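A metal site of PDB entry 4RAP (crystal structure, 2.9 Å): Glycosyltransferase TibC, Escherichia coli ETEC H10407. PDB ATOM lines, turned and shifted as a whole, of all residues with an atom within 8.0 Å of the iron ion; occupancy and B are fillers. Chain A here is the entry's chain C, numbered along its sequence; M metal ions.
The backbone carbonyl oxygen of Phe 320 lies within hydrogen-bond range of the backbone NH of Cys 342 (3.0 Å). The side-chain sulfur (SG) of Cys 339 sits close to the guanidinium group (NH1) of Arg 360. The backbone NH (N) of Cys 339 sits at hydrogen-bond distance from the side-chain carboxylate (OE1) of Glu 369 (3.0 Å). The side-chain sulfur (SG) of Cys 358 is in hydrogen-bond range of the backbone NH (N) of Phe 368 (3.8 Å).
Of the 22 residues printed, 4 come within 4 Å of the iron ion. The nearest printed residue that does not touch the iron ion is His 361 (4.9 Å).
The iron ion is bound by SG of Cys 370, SG of Cys 342 and SG of Cys 339. The iron ion has three donor atoms within binding distance. Slightly farther from the iron ion lies SG of Cys 358 (2.9 Å).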
ATOM      1  N   ALA A 229      14.320 -26.895  30.448  1.00  0.00           N
ATOM      2  CA  ALA A 229      14.181 -26.099  29.207  1.00  0.00           C
ATOM      3  C   ALA A 229      14.102 -24.623  29.498  1.00  0.00           C
ATOM      4  O   ALA A 229      14.467 -23.831  28.643  1.00  0.00           O
ATOM      5  CB  ALA A 229      12.967 -26.545  28.392  1.00  0.00           C
ATOM      6  N   GLY A 319      14.017 -19.165  25.429  1.00  0.00           N
ATOM      7  CA  GLY A 319      13.909 -19.722  24.068  1.00  0.00           C
ATOM      8  C   GLY A 319      12.813 -20.793  23.914  1.00  0.00           C
ATOM      9  O   GLY A 319      12.348 -21.074  22.826  1.00  0.00           O
ATOM     10  N   PHE A 320      12.357 -21.368  25.015  1.00  0.00           N
ATOM     11  CA  PHE A 320      11.355 -22.396  24.910  1.00  0.00           C
ATOM     12  C   PHE A 320       9.970 -21.848  24.724  1.00  0.00           C
ATOM     13  O   PHE A 320       9.064 -22.562  24.327  1.00  0.00           O
ATOM     14  CB  PHE A 320      11.475 -23.416  26.021  1.00  0.00           C
ATOM     15  CG  PHE A 320      10.424 -23.341  27.057  1.00  0.00           C
ATOM     16  CD1 PHE A 320      10.166 -22.167  27.731  1.00  0.00           C
ATOM     17  CD2 PHE A 320       9.777 -24.494  27.478  1.00  0.00           C
ATOM     18  CE1 PHE A 320       9.221 -22.125  28.743  1.00  0.00           C
ATOM     19  CE2 PHE A 320       8.836 -24.461  28.492  1.00  0.00           C
ATOM     20  CZ  PHE A 320       8.566 -23.266  29.133  1.00  0.00           C
ATOM     21  N   GLY A 338      17.115 -21.390  15.349  1.00  0.00           N
ATOM     22  CA  GLY A 338      17.053 -22.849  15.553  1.00  0.00           C
ATOM     23  C   GLY A 338      15.691 -23.241  16.083  1.00  0.00           C
ATOM     24  O   GLY A 338      14.726 -22.572  15.735  1.00  0.00           O
ATOM     25  N   CYS A 339      15.595 -24.330  16.893  1.00  0.00           N
ATOM     26  CA  CYS A 339      14.313 -24.709  17.585  1.00  0.00           C
ATOM     27  C   CYS A 339      14.014 -23.552  18.565  1.00  0.00           C
ATOM     28  O   CYS A 339      14.932 -22.908  19.091  1.00  0.00           O
ATOM     29  CB  CYS A 339      14.346 -26.183  18.238  1.00  0.00           C
ATOM     30  SG  CYS A 339      13.365 -26.727  19.789  1.00  0.00           S
ATOM     31  N   TYR A 340      12.745 -23.186  18.667  1.00  0.00           N
ATOM     32  CA  TYR A 340      12.283 -22.293  19.720  1.00  0.00           C
ATOM     33  C   TYR A 340      10.770 -22.532  19.954  1.00  0.00           C
ATOM     34  O   TYR A 340      10.090 -23.178  19.125  1.00  0.00           O
ATOM     35  CB  TYR A 340      12.537 -20.877  19.351  1.00  0.00           C
ATOM     36  CG  TYR A 340      11.873 -20.480  18.074  1.00  0.00           C
ATOM     37  CD1 TYR A 340      10.477 -20.387  17.999  1.00  0.00           C
ATOM     38  CD2 TYR A 340      12.631 -20.186  16.933  1.00  0.00           C
ATOM     39  CE1 TYR A 340       9.856 -20.030  16.816  1.00  0.00           C
ATOM     40  CE2 TYR A 340      12.017 -19.792  15.751  1.00  0.00           C
ATOM     41  CZ  TYR A 340      10.625 -19.738  15.697  1.00  0.00           C
ATOM     42  OH  TYR A 340       9.993 -19.371  14.534  1.00  0.00           O
ATOM     43  N   GLY A 341      10.262 -22.103  21.098  1.00  0.00           N
ATOM     44  CA  GLY A 341       8.827 -22.201  21.348  1.00  0.00           C
ATOM     45  C   GLY A 341       8.177 -23.568  21.538  1.00  0.00           C
ATOM     46  O   GLY A 341       7.019 -23.725  21.214  1.00  0.00           O
ATOM     47  N   CYS A 342       8.926 -24.557  22.035  1.00  0.00           N
ATOM     48  CA  CYS A 342       8.405 -25.883  22.475  1.00  0.00           C
ATOM     49  C   CYS A 342       7.016 -25.569  23.127  1.00  0.00           C
ATOM     50  O   CYS A 342       5.964 -26.033  22.697  1.00  0.00           O
ATOM     51  CB  CYS A 342       9.438 -26.611  23.518  1.00  0.00           C
ATOM     52  SG  CYS A 342      11.289 -26.683  23.055  1.00  0.00           S
ATOM     53  N   TRP A 343       7.043 -24.653  24.095  1.00  0.00           N
ATOM     54  CA  TRP A 343       5.940 -24.403  25.003  1.00  0.00           C
ATOM     55  C   TRP A 343       4.646 -23.899  24.422  1.00  0.00           C
ATOM     56  O   TRP A 343       3.573 -24.189  24.952  1.00  0.00           O
ATOM     57  CB  TRP A 343       6.452 -23.451  26.083  1.00  0.00           C
ATOM     58  CG  TRP A 343       5.387 -22.893  26.982  1.00  0.00           C
ATOM     59  CD1 TRP A 343       4.749 -21.656  26.868  1.00  0.00           C
ATOM     60  CD2 TRP A 343       4.795 -23.527  28.167  1.00  0.00           C
ATOM     61  NE1 TRP A 343       3.843 -21.494  27.885  1.00  0.00           N
ATOM     62  CE2 TRP A 343       3.831 -22.576  28.700  1.00  0.00           C
ATOM     63  CE3 TRP A 343       4.958 -24.742  28.798  1.00  0.00           C
ATOM     64  CZ2 TRP A 343       3.058 -22.857  29.832  1.00  0.00           C
ATOM     65  CZ3 TRP A 343       4.192 -25.018  29.936  1.00  0.00           C
ATOM     66  CH2 TRP A 343       3.253 -24.097  30.432  1.00  0.00           C
ATOM     67  N   LEU A 348       2.325 -30.219  20.171  1.00  0.00           N
ATOM     68  CA  LEU A 348       3.157 -30.927  21.168  1.00  0.00           C
ATOM     69  C   LEU A 348       2.456 -30.908  22.515  1.00  0.00           C
ATOM     70  O   LEU A 348       1.437 -30.262  22.647  1.00  0.00           O
ATOM     71  CB  LEU A 348       4.507 -30.237  21.287  1.00  0.00           C
ATOM     72  CG  LEU A 348       5.279 -30.222  19.940  1.00  0.00           C
ATOM     73  CD1 LEU A 348       6.579 -29.426  20.038  1.00  0.00           C
ATOM     74  CD2 LEU A 348       5.532 -31.643  19.451  1.00  0.00           C
ATOM     75  N   TRP A 357      12.460 -32.460  29.650  1.00  0.00           N
ATOM     76  CA  TRP A 357      11.566 -32.369  28.513  1.00  0.00           C
ATOM     77  C   TRP A 357      12.114 -31.490  27.368  1.00  0.00           C
ATOM     78  O   TRP A 357      12.525 -30.365  27.616  1.00  0.00           O
ATOM     79  CB  TRP A 357      10.234 -31.867  29.014  1.00  0.00           C
ATOM     80  CG  TRP A 357       9.155 -31.712  27.959  1.00  0.00           C
ATOM     81  CD1 TRP A 357       8.461 -32.725  27.295  1.00  0.00           C
ATOM     82  CD2 TRP A 357       8.553 -30.462  27.468  1.00  0.00           C
ATOM     83  NE1 TRP A 357       7.527 -32.197  26.427  1.00  0.00           N
ATOM     84  CE2 TRP A 357       7.531 -30.848  26.496  1.00  0.00           C
ATOM     85  CE3 TRP A 357       8.767 -29.124  27.726  1.00  0.00           C
ATOM     86  CZ2 TRP A 357       6.760 -29.915  25.822  1.00  0.00           C
ATOM     87  CZ3 TRP A 357       7.985 -28.187  27.044  1.00  0.00           C
ATOM     88  CH2 TRP A 357       7.002 -28.579  26.117  1.00  0.00           C
ATOM     89  N   CYS A 358      12.216 -32.065  26.168  1.00  0.00           N
ATOM     90  CA  CYS A 358      12.540 -31.368  24.915  1.00  0.00           C
ATOM     91  C   CYS A 358      11.880 -32.175  23.778  1.00  0.00           C
ATOM     92  O   CYS A 358      12.548 -33.025  23.147  1.00  0.00           O
ATOM     93  CB  CYS A 358      14.063 -31.218  24.604  1.00  0.00           C
ATOM     94  SG  CYS A 358      14.483 -29.902  23.360  1.00  0.00           S
ATOM     95  N   PRO A 359      10.586 -31.889  23.470  1.00  0.00           N
ATOM     96  CA  PRO A 359       9.852 -32.685  22.512  1.00  0.00           C
ATOM     97  C   PRO A 359      10.543 -32.882  21.199  1.00  0.00           C
ATOM     98  O   PRO A 359      10.410 -33.927  20.632  1.00  0.00           O
ATOM     99  CB  PRO A 359       8.563 -31.911  22.282  1.00  0.00           C
ATOM    100  CG  PRO A 359       8.594 -30.732  23.148  1.00  0.00           C
ATOM    101  CD  PRO A 359       9.807 -30.763  23.997  1.00  0.00           C
ATOM    102  N   ARG A 360      11.252 -31.884  20.692  1.00  0.00           N
ATOM    103  CA  ARG A 360      11.841 -32.034  19.343  1.00  0.00           C
ATOM    104  C   ARG A 360      13.265 -32.537  19.317  1.00  0.00           C
ATOM    105  O   ARG A 360      13.679 -33.074  18.310  1.00  0.00           O
ATOM    106  CB  ARG A 360      11.729 -30.774  18.472  1.00  0.00           C
ATOM    107  CG  ARG A 360      10.328 -30.158  18.446  1.00  0.00           C
ATOM    108  CD  ARG A 360      10.216 -29.012  17.447  1.00  0.00           C
ATOM    109  NE  ARG A 360       9.074 -28.120  17.698  1.00  0.00           N
ATOM    110  CZ  ARG A 360       9.200 -26.851  18.106  1.00  0.00           C
ATOM    111  NH1 ARG A 360      10.406 -26.333  18.266  1.00  0.00           N
ATOM    112  NH2 ARG A 360       8.127 -26.078  18.272  1.00  0.00           N
ATOM    113  N   HIS A 361      14.008 -32.405  20.412  1.00  0.00           N
ATOM    114  CA  HIS A 361      15.426 -32.776  20.383  1.00  0.00           C
ATOM    115  C   HIS A 361      15.966 -33.545  21.545  1.00  0.00           C
ATOM    116  O   HIS A 361      17.176 -33.756  21.637  1.00  0.00           O
ATOM    117  CB  HIS A 361      16.302 -31.570  20.087  1.00  0.00           C
ATOM    118  CG  HIS A 361      16.033 -30.957  18.737  1.00  0.00           C
ATOM    119  ND1 HIS A 361      15.303 -29.837  18.589  1.00  0.00           N
ATOM    120  CD2 HIS A 361      16.338 -31.395  17.459  1.00  0.00           C
ATOM    121  CE1 HIS A 361      15.206 -29.527  17.283  1.00  0.00           C
ATOM    122  NE2 HIS A 361      15.825 -30.491  16.588  1.00  0.00           N
ATOM    123  N   LYS A 362      15.106 -33.988  22.449  1.00  0.00           N
ATOM    124  CA  LYS A 362      15.560 -34.779  23.587  1.00  0.00           C
ATOM    125  C   LYS A 362      16.521 -35.890  23.163  1.00  0.00           C
ATOM    126  O   LYS A 362      16.306 -36.553  22.155  1.00  0.00           O
ATOM    127  CB  LYS A 362      14.383 -35.371  24.377  1.00  0.00           C
ATOM    128  CG  LYS A 362      14.826 -36.255  25.526  1.00  0.00           C
ATOM    129  CD  LYS A 362      13.763 -36.460  26.587  1.00  0.00           C
ATOM    130  CE  LYS A 362      14.424 -36.938  27.858  1.00  0.00           C
ATOM    131  NZ  LYS A 362      13.452 -37.256  28.933  1.00  0.00           N
ATOM    132  N   ARG A 366      21.137 -31.554  19.741  1.00  0.00           N
ATOM    133  CA  ARG A 366      20.460 -30.294  19.666  1.00  0.00           C
ATOM    134  C   ARG A 366      19.577 -30.041  20.868  1.00  0.00           C
ATOM    135  O   ARG A 366      18.888 -29.015  20.946  1.00  0.00           O
ATOM    136  CB  ARG A 366      19.644 -30.249  18.387  1.00  0.00           C
ATOM    137  CG  ARG A 366      20.476 -30.434  17.143  1.00  0.00           C
ATOM    138  CD  ARG A 366      19.623 -30.390  15.886  1.00  0.00           C
ATOM    139  NE  ARG A 366      19.043 -29.075  15.692  1.00  0.00           N
ATOM    140  CZ  ARG A 366      18.076 -28.823  14.805  1.00  0.00           C
ATOM    141  NH1 ARG A 366      17.619 -29.812  14.041  1.00  0.00           N
ATOM    142  NH2 ARG A 366      17.582 -27.597  14.692  1.00  0.00           N
ATOM    143  N   GLN A 367      19.630 -30.937  21.855  1.00  0.00           N
ATOM    144  CA  GLN A 367      18.832 -30.740  23.024  1.00  0.00           C
ATOM    145  C   GLN A 367      19.081 -29.374  23.637  1.00  0.00           C
ATOM    146  O   GLN A 367      20.212 -28.970  23.855  1.00  0.00           O
ATOM    147  CB  GLN A 367      19.102 -31.820  24.039  1.00  0.00           C
ATOM    148  CG  GLN A 367      18.123 -31.810  25.202  1.00  0.00           C
ATOM    149  CD  GLN A 367      18.111 -33.135  25.927  1.00  0.00           C
ATOM    150  OE1 GLN A 367      18.886 -34.021  25.605  1.00  0.00           O
ATOM    151  NE2 GLN A 367      17.225 -33.286  26.897  1.00  0.00           N
ATOM    152  N   PHE A 368      17.999 -28.665  23.901  1.00  0.00           N
ATOM    153  CA  PHE A 368      18.031 -27.340  24.479  1.00  0.00           C
ATOM    154  C   PHE A 368      18.666 -26.230  23.627  1.00  0.00           C
ATOM    155  O   PHE A 368      19.053 -25.187  24.143  1.00  0.00           O
ATOM    156  CB  PHE A 368      18.530 -27.359  25.907  1.00  0.00           C
ATOM    157  CG  PHE A 368      17.746 -28.284  26.803  1.00  0.00           C
ATOM    158  CD1 PHE A 368      16.369 -28.270  26.793  1.00  0.00           C
ATOM    159  CD2 PHE A 368      18.409 -29.137  27.693  1.00  0.00           C
ATOM    160  CE1 PHE A 368      15.649 -29.114  27.602  1.00  0.00           C
ATOM    161  CE2 PHE A 368      17.695 -29.971  28.535  1.00  0.00           C
ATOM    162  CZ  PHE A 368      16.301 -29.963  28.483  1.00  0.00           C
ATOM    163  N   GLU A 369      18.740 -26.457  22.316  1.00  0.00           N
ATOM    164  CA  GLU A 369      19.143 -25.443  21.354  1.00  0.00           C
ATOM    165  C   GLU A 369      18.340 -24.152  21.576  1.00  0.00           C
ATOM    166  O   GLU A 369      18.754 -23.078  21.193  1.00  0.00           O
ATOM    167  CB  GLU A 369      18.835 -25.978  19.961  1.00  0.00           C
ATOM    168  CG  GLU A 369      19.825 -25.528  18.889  1.00  0.00           C
ATOM    169  CD  GLU A 369      19.428 -25.968  17.507  1.00  0.00           C
ATOM    170  OE1 GLU A 369      18.278 -25.713  17.089  1.00  0.00           O
ATOM    171  OE2 GLU A 369      20.286 -26.527  16.819  1.00  0.00           O
ATOM    172  N   CYS A 370      17.159 -24.311  22.175  1.00  0.00           N
ATOM    173  CA  CYS A 370      16.258 -23.209  22.528  1.00  0.00           C
ATOM    174  C   CYS A 370      17.169 -22.034  23.037  1.00  0.00           C
ATOM    175  O   CYS A 370      17.082 -20.922  22.556  1.00  0.00           O
ATOM    176  CB  CYS A 370      15.187 -23.714  23.625  1.00  0.00           C
ATOM    177  SG  CYS A 370      14.230 -25.326  23.345  1.00  0.00           S
ATOM    178  N   THR A 371      18.107 -22.342  23.928  1.00  0.00           N
ATOM    179  CA  THR A 371      18.825 -21.344  24.688  1.00  0.00           C
ATOM    180  C   THR A 371      20.350 -21.434  24.582  1.00  0.00           C
ATOM    181  O   THR A 371      21.070 -20.509  25.012  1.00  0.00           O
ATOM    182  CB  THR A 371      18.431 -21.390  26.176  1.00  0.00           C
ATOM    183  OG1 THR A 371      18.588 -22.721  26.685  1.00  0.00           O
ATOM    184  CG2 THR A 371      17.008 -21.018  26.334  1.00  0.00           C
HETATM  185 FE    FE M   1      13.464 -27.324  22.404  1.00  0.00          FE
